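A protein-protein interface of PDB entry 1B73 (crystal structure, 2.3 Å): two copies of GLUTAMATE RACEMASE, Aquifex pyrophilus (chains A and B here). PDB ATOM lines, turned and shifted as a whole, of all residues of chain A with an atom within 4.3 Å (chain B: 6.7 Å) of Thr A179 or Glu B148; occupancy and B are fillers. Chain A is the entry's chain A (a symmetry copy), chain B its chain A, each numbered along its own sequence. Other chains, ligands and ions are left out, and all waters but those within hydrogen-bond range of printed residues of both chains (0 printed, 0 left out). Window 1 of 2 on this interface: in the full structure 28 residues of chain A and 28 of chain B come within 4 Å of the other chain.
The backbone NH of Ala B143 sits close to the side-chain carboxylate of Glu B148 (3.3 Å).
The backbone carbonyl oxygen (O) of Leu B151 sits at hydrogen-bond distance from the side-chain hydroxyl (OH) of Tyr B181, 3.4 Å away.
The side-chain hydroxyl (OG1) of Thr A179 sits at hydrogen-bond distance from the backbone carbonyl oxygen (O) of Leu A183 (3.1 Å).
Of the 15 printed residues of chain B, 5 touch a printed residue of chain A.
Hydrophobic or aromatic side chains of chain B within 4 Å of the printed part of chain A: Tyr B181.
Of the 7 printed residues of chain A, 6 touch a printed residue of chain B.
Among the printed residues, 9 pairs touch across the chains.
Among the printed residues, no Asp or Glu carboxylate lies within 4 Å of a Lys or Arg side-chain nitrogen of the other chain.
The backbone NH (N) of Thr A179 is in hydrogen-bond range of the side-chain carboxylate (OE2) of Glu B147 (3.2 Å).
O of Thr A179 lies within hydrogen-bond range of N of Gly B149 (3.1 Å).
The side-chain carboxylate of Glu B152 is in hydrogen-bond range of the backbone NH of Lys A185 (2.9 Å).
Cys A178 touches Glu B147.
Glu B148 touches Thr A179.
Glu B147 touches His A180.
Tyr B181 touches Tyr A181 (CD1 to CD1, 3.4 Å).
Leu A184 touches Glu B152.
Leu A184 touches Tyr B181.
Tyr A181 touches its own counterpart, Tyr B181.
2 positions are printed for both chains.
Of the 9 pairs that touch across the chains among the printed residues, 1 has its exchanged pair printed and touching as well.
Printed residues of chain A within 4 Å of Glu B147: Cys A178, Thr A179 and His A180.
Printed residues of chain B within 4 Å of His A180: Glu B147.
Printed residues of chain A within 4 Å of Tyr B181: Tyr A181 and Leu A184.
Of the printed residues of chain B, Lys A185 touches Glu B152.
Of the printed residues of chain A, Glu B152 touches Leu A184 and Lys A185.
Leu B150 touches none of the printed residues of chain A.
Leu A183 touches none of the printed residues of chain B.
The nearest printed residue of chain B that does not touch Thr A179 is Glu B152 (4.9 Å).
The nearest printed residue of chain A that does not touch Glu B152 is Thr A179 (4.9 Å).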
ATOM      1  N   CYS A 178      34.096 -22.117   2.990  1.00  0.00           N
ATOM      2  CA  CYS A 178      32.846 -21.418   2.805  1.00  0.00           C
ATOM      3  C   CYS A 178      32.317 -21.505   1.392  1.00  0.00           C
ATOM      4  O   CYS A 178      32.923 -20.977   0.465  1.00  0.00           O
ATOM      5  CB  CYS A 178      33.059 -20.001   3.261  1.00  0.00           C
ATOM      6  SG  CYS A 178      33.692 -20.072   4.933  1.00  0.00           S
ATOM      7  N   THR A 179      31.148 -22.123   1.265  1.00  0.00           N
ATOM      8  CA  THR A 179      30.514 -22.349  -0.026  1.00  0.00           C
ATOM      9  C   THR A 179      29.589 -21.301  -0.652  1.00  0.00           C
ATOM     10  O   THR A 179      28.478 -21.069  -0.182  1.00  0.00           O
ATOM     11  CB  THR A 179      29.782 -23.711  -0.039  1.00  0.00           C
ATOM     12  OG1 THR A 179      28.851 -23.738  -1.122  1.00  0.00           O
ATOM     13  CG2 THR A 179      29.046 -23.942   1.276  1.00  0.00           C
ATOM     14  N   HIS A 180      30.019 -20.753  -1.782  1.00  0.00           N
ATOM     15  CA  HIS A 180      29.245 -19.770  -2.533  1.00  0.00           C
ATOM     16  C   HIS A 180      29.026 -20.237  -3.951  1.00  0.00           C
ATOM     17  O   HIS A 180      29.924 -20.805  -4.565  1.00  0.00           O
ATOM     18  CB  HIS A 180      29.986 -18.454  -2.628  1.00  0.00           C
ATOM     19  CG  HIS A 180      29.702 -17.526  -1.510  1.00  0.00           C
ATOM     20  ND1 HIS A 180      30.520 -16.467  -1.202  1.00  0.00           N
ATOM     21  CD2 HIS A 180      28.699 -17.514  -0.602  1.00  0.00           C
ATOM     22  CE1 HIS A 180      30.044 -15.843  -0.143  1.00  0.00           C
ATOM     23  NE2 HIS A 180      28.942 -16.458   0.241  1.00  0.00           N
ATOM     24  N   TYR A 181      27.867 -19.871  -4.502  1.00  0.00           N
ATOM     25  CA  TYR A 181      27.500 -20.221  -5.864  1.00  0.00           C
ATOM     26  C   TYR A 181      28.512 -19.648  -6.867  1.00  0.00           C
ATOM     27  O   TYR A 181      28.941 -18.494  -6.743  1.00  0.00           O
ATOM     28  CB  TYR A 181      26.076 -19.718  -6.182  1.00  0.00           C
ATOM     29  CG  TYR A 181      25.517 -20.391  -7.406  1.00  0.00           C
ATOM     30  CD1 TYR A 181      24.905 -21.646  -7.320  1.00  0.00           C
ATOM     31  CD2 TYR A 181      25.720 -19.850  -8.666  1.00  0.00           C
ATOM     32  CE1 TYR A 181      24.525 -22.346  -8.466  1.00  0.00           C
ATOM     33  CE2 TYR A 181      25.355 -20.542  -9.815  1.00  0.00           C
ATOM     34  CZ  TYR A 181      24.760 -21.788  -9.704  1.00  0.00           C
ATOM     35  OH  TYR A 181      24.405 -22.477 -10.844  1.00  0.00           O
ATOM     36  N   LEU A 183      30.084 -22.633  -6.573  1.00  0.00           N
ATOM     37  CA  LEU A 183      30.854 -23.652  -5.874  1.00  0.00           C
ATOM     38  C   LEU A 183      30.078 -24.331  -4.780  1.00  0.00           C
ATOM     39  O   LEU A 183      30.528 -24.426  -3.637  1.00  0.00           O
ATOM     40  CB  LEU A 183      32.149 -23.070  -5.294  1.00  0.00           C
ATOM     41  CG  LEU A 183      33.210 -22.633  -6.296  1.00  0.00           C
ATOM     42  CD1 LEU A 183      34.511 -22.388  -5.547  1.00  0.00           C
ATOM     43  CD2 LEU A 183      33.397 -23.727  -7.332  1.00  0.00           C
ATOM     44  N   LEU A 184      28.889 -24.813  -5.114  1.00  0.00           N
ATOM     45  CA  LEU A 184      28.091 -25.483  -4.108  1.00  0.00           C
ATOM     46  C   LEU A 184      28.808 -26.787  -3.797  1.00  0.00           C
ATOM     47  O   LEU A 184      29.735 -27.146  -4.513  1.00  0.00           O
ATOM     48  CB  LEU A 184      26.706 -25.785  -4.676  1.00  0.00           C
ATOM     49  CG  LEU A 184      25.864 -24.624  -5.208  1.00  0.00           C
ATOM     50  CD1 LEU A 184      24.486 -25.188  -5.531  1.00  0.00           C
ATOM     51  CD2 LEU A 184      25.736 -23.483  -4.171  1.00  0.00           C
ATOM     52  N   LYS A 185      28.380 -27.487  -2.749  1.00  0.00           N
ATOM     53  CA  LYS A 185      28.966 -28.779  -2.376  1.00  0.00           C
ATOM     54  C   LYS A 185      28.834 -29.786  -3.534  1.00  0.00           C
ATOM     55  O   LYS A 185      29.813 -30.399  -3.923  1.00  0.00           O
ATOM     56  CB  LYS A 185      28.293 -29.318  -1.114  1.00  0.00           C
ATOM     57  CG  LYS A 185      28.881 -30.624  -0.542  1.00  0.00           C
ATOM     58  CD  LYS A 185      28.129 -31.028   0.731  1.00  0.00           C
ATOM     59  CE  LYS A 185      28.621 -32.347   1.327  1.00  0.00           C
ATOM     60  NZ  LYS A 185      28.059 -33.574   0.657  1.00  0.00           N
ATOM     61  N   PRO B 140      14.755 -13.319  -3.610  1.00  0.00           N
ATOM     62  CA  PRO B 140      15.135 -13.426  -2.188  1.00  0.00           C
ATOM     63  C   PRO B 140      16.601 -13.002  -2.094  1.00  0.00           C
ATOM     64  O   PRO B 140      17.435 -13.529  -2.829  1.00  0.00           O
ATOM     65  CB  PRO B 140      15.004 -14.918  -1.905  1.00  0.00           C
ATOM     66  CG  PRO B 140      15.421 -15.557  -3.204  1.00  0.00           C
ATOM     67  CD  PRO B 140      14.684 -14.659  -4.232  1.00  0.00           C
ATOM     68  N   LEU B 141      16.907 -12.003  -1.268  1.00  0.00           N
ATOM     69  CA  LEU B 141      18.287 -11.536  -1.142  1.00  0.00           C
ATOM     70  C   LEU B 141      18.988 -12.385  -0.075  1.00  0.00           C
ATOM     71  O   LEU B 141      19.018 -12.017   1.095  1.00  0.00           O
ATOM     72  CB  LEU B 141      18.345 -10.050  -0.720  1.00  0.00           C
ATOM     73  CG  LEU B 141      17.311  -8.914  -0.904  1.00  0.00           C
ATOM     74  CD1 LEU B 141      17.192  -8.489  -2.352  1.00  0.00           C
ATOM     75  CD2 LEU B 141      15.966  -9.265  -0.294  1.00  0.00           C
ATOM     76  N   PHE B 142      19.618 -13.479  -0.478  1.00  0.00           N
ATOM     77  CA  PHE B 142      20.254 -14.341   0.499  1.00  0.00           C
ATOM     78  C   PHE B 142      21.743 -14.291   0.805  1.00  0.00           C
ATOM     79  O   PHE B 142      22.102 -14.328   1.970  1.00  0.00           O
ATOM     80  CB  PHE B 142      19.816 -15.791   0.275  1.00  0.00           C
ATOM     81  CG  PHE B 142      18.375 -16.066   0.658  1.00  0.00           C
ATOM     82  CD1 PHE B 142      17.781 -15.413   1.720  1.00  0.00           C
ATOM     83  CD2 PHE B 142      17.637 -17.031  -0.016  1.00  0.00           C
ATOM     84  CE1 PHE B 142      16.481 -15.721   2.108  1.00  0.00           C
ATOM     85  CE2 PHE B 142      16.348 -17.340   0.367  1.00  0.00           C
ATOM     86  CZ  PHE B 142      15.769 -16.679   1.437  1.00  0.00           C
ATOM     87  N   ALA B 143      22.604 -14.177  -0.208  1.00  0.00           N
ATOM     88  CA  ALA B 143      24.057 -14.189   0.012  1.00  0.00           C
ATOM     89  C   ALA B 143      24.633 -13.337   1.129  1.00  0.00           C
ATOM     90  O   ALA B 143      25.599 -13.754   1.773  1.00  0.00           O
ATOM     91  CB  ALA B 143      24.832 -13.956  -1.278  1.00  0.00           C
ATOM     92  N   PRO B 144      24.084 -12.124   1.363  1.00  0.00           N
ATOM     93  CA  PRO B 144      24.619 -11.282   2.448  1.00  0.00           C
ATOM     94  C   PRO B 144      24.572 -12.016   3.790  1.00  0.00           C
ATOM     95  O   PRO B 144      25.619 -12.307   4.354  1.00  0.00           O
ATOM     96  CB  PRO B 144      23.671 -10.078   2.448  1.00  0.00           C
ATOM     97  CG  PRO B 144      23.272  -9.974   0.995  1.00  0.00           C
ATOM     98  CD  PRO B 144      23.034 -11.413   0.607  1.00  0.00           C
ATOM     99  N   ALA B 146      23.397 -15.344   4.717  1.00  0.00           N
ATOM    100  CA  ALA B 146      23.906 -16.689   4.707  1.00  0.00           C
ATOM    101  C   ALA B 146      24.434 -17.060   3.355  1.00  0.00           C
ATOM    102  O   ALA B 146      23.909 -16.636   2.326  1.00  0.00           O
ATOM    103  CB  ALA B 146      22.819 -17.660   5.093  1.00  0.00           C
ATOM    104  N   GLU B 147      25.436 -17.930   3.383  1.00  0.00           N
ATOM    105  CA  GLU B 147      26.077 -18.439   2.188  1.00  0.00           C
ATOM    106  C   GLU B 147      25.131 -19.389   1.504  1.00  0.00           C
ATOM    107  O   GLU B 147      24.471 -20.203   2.144  1.00  0.00           O
ATOM    108  CB  GLU B 147      27.392 -19.119   2.541  1.00  0.00           C
ATOM    109  CG  GLU B 147      28.433 -18.117   2.998  1.00  0.00           C
ATOM    110  CD  GLU B 147      29.744 -18.755   3.370  1.00  0.00           C
ATOM    111  OE1 GLU B 147      30.676 -18.019   3.688  1.00  0.00           O
ATOM    112  OE2 GLU B 147      29.860 -19.994   3.330  1.00  0.00           O
ATOM    113  N   GLU B 148      25.054 -19.255   0.191  1.00  0.00           N
ATOM    114  CA  GLU B 148      24.168 -20.077  -0.618  1.00  0.00           C
ATOM    115  C   GLU B 148      24.338 -21.566  -0.340  1.00  0.00           C
ATOM    116  O   GLU B 148      23.371 -22.317  -0.387  1.00  0.00           O
ATOM    117  CB  GLU B 148      24.377 -19.743  -2.094  1.00  0.00           C
ATOM    118  CG  GLU B 148      24.689 -18.258  -2.348  1.00  0.00           C
ATOM    119  CD  GLU B 148      23.557 -17.289  -1.949  1.00  0.00           C
ATOM    120  OE1 GLU B 148      22.895 -17.482  -0.903  1.00  0.00           O
ATOM    121  OE2 GLU B 148      23.348 -16.297  -2.687  1.00  0.00           O
ATOM    122  N   GLY B 149      25.549 -21.971   0.041  1.00  0.00           N
ATOM    123  CA  GLY B 149      25.819 -23.373   0.342  1.00  0.00           C
ATOM    124  C   GLY B 149      24.935 -23.890   1.460  1.00  0.00           C
ATOM    125  O   GLY B 149      24.814 -25.097   1.682  1.00  0.00           O
ATOM    126  N   LEU B 150      24.351 -22.959   2.202  1.00  0.00           N
ATOM    127  CA  LEU B 150      23.435 -23.305   3.273  1.00  0.00           C
ATOM    128  C   LEU B 150      22.136 -23.731   2.592  1.00  0.00           C
ATOM    129  O   LEU B 150      21.526 -24.736   2.953  1.00  0.00           O
ATOM    130  CB  LEU B 150      23.173 -22.075   4.145  1.00  0.00           C
ATOM    131  CG  LEU B 150      22.030 -22.179   5.154  1.00  0.00           C
ATOM    132  CD1 LEU B 150      22.475 -22.946   6.400  1.00  0.00           C
ATOM    133  CD2 LEU B 150      21.562 -20.773   5.517  1.00  0.00           C
ATOM    134  N   LEU B 151      21.774 -22.980   1.554  1.00  0.00           N
ATOM    135  CA  LEU B 151      20.555 -23.205   0.792  1.00  0.00           C
ATOM    136  C   LEU B 151      20.619 -24.367  -0.193  1.00  0.00           C
ATOM    137  O   LEU B 151      19.830 -24.430  -1.142  1.00  0.00           O
ATOM    138  CB  LEU B 151      20.168 -21.920   0.056  1.00  0.00           C
ATOM    139  CG  LEU B 151      19.921 -20.666   0.902  1.00  0.00           C
ATOM    140  CD1 LEU B 151      19.613 -21.051   2.327  1.00  0.00           C
ATOM    141  CD2 LEU B 151      21.116 -19.750   0.866  1.00  0.00           C
ATOM    142  N   GLU B 152      21.534 -25.297   0.033  1.00  0.00           N
ATOM    143  CA  GLU B 152      21.671 -26.434  -0.875  1.00  0.00           C
ATOM    144  C   GLU B 152      20.905 -27.635  -0.351  1.00  0.00           C
ATOM    145  O   GLU B 152      20.859 -27.861   0.853  1.00  0.00           O
ATOM    146  CB  GLU B 152      23.149 -26.778  -1.078  1.00  0.00           C
ATOM    147  CG  GLU B 152      23.429 -27.778  -2.195  1.00  0.00           C
ATOM    148  CD  GLU B 152      24.914 -28.031  -2.368  1.00  0.00           C
ATOM    149  OE1 GLU B 152      25.304 -28.852  -3.236  1.00  0.00           O
ATOM    150  OE2 GLU B 152      25.693 -27.395  -1.615  1.00  0.00           O
ATOM    151  N   HIS B 180      18.215 -15.266  -8.758  1.00  0.00           N
ATOM    152  CA  HIS B 180      19.174 -15.422  -7.670  1.00  0.00           C
ATOM    153  C   HIS B 180      18.991 -16.754  -6.986  1.00  0.00           C
ATOM    154  O   HIS B 180      17.865 -17.200  -6.786  1.00  0.00           O
ATOM    155  CB  HIS B 180      18.964 -14.364  -6.608  1.00  0.00           C
ATOM    156  CG  HIS B 180      19.733 -13.122  -6.840  1.00  0.00           C
ATOM    157  ND1 HIS B 180      19.419 -11.932  -6.231  1.00  0.00           N
ATOM    158  CD2 HIS B 180      20.795 -12.875  -7.642  1.00  0.00           C
ATOM    159  CE1 HIS B 180      20.244 -10.995  -6.653  1.00  0.00           C
ATOM    160  NE2 HIS B 180      21.087 -11.539  -7.510  1.00  0.00           N
ATOM    161  N   TYR B 181      20.106 -17.315  -6.514  1.00  0.00           N
ATOM    162  CA  TYR B 181      20.110 -18.587  -5.814  1.00  0.00           C
ATOM    163  C   TYR B 181      19.242 -18.519  -4.549  1.00  0.00           C
ATOM    164  O   TYR B 181      19.290 -17.534  -3.801  1.00  0.00           O
ATOM    165  CB  TYR B 181      21.553 -19.000  -5.459  1.00  0.00           C
ATOM    166  CG  TYR B 181      21.635 -20.461  -5.105  1.00  0.00           C
ATOM    167  CD1 TYR B 181      21.749 -21.437  -6.102  1.00  0.00           C
ATOM    168  CD2 TYR B 181      21.459 -20.883  -3.797  1.00  0.00           C
ATOM    169  CE1 TYR B 181      21.667 -22.796  -5.795  1.00  0.00           C
ATOM    170  CE2 TYR B 181      21.367 -22.232  -3.481  1.00  0.00           C
ATOM    171  CZ  TYR B 181      21.471 -23.179  -4.486  1.00  0.00           C
ATOM    172  OH  TYR B 181      21.372 -24.519  -4.173  1.00  0.00           O
ATOM    173  N   PRO B 182      18.440 -19.571  -4.276  1.00  0.00           N
ATOM    174  CA  PRO B 182      18.249 -20.848  -4.985  1.00  0.00           C
ATOM    175  C   PRO B 182      17.249 -20.845  -6.155  1.00  0.00           C
ATOM    176  O   PRO B 182      16.923 -21.923  -6.704  1.00  0.00           O
ATOM    177  CB  PRO B 182      17.720 -21.738  -3.882  1.00  0.00           C
ATOM    178  CG  PRO B 182      16.788 -20.810  -3.181  1.00  0.00           C
ATOM    179  CD  PRO B 182      17.683 -19.589  -3.008  1.00  0.00           C
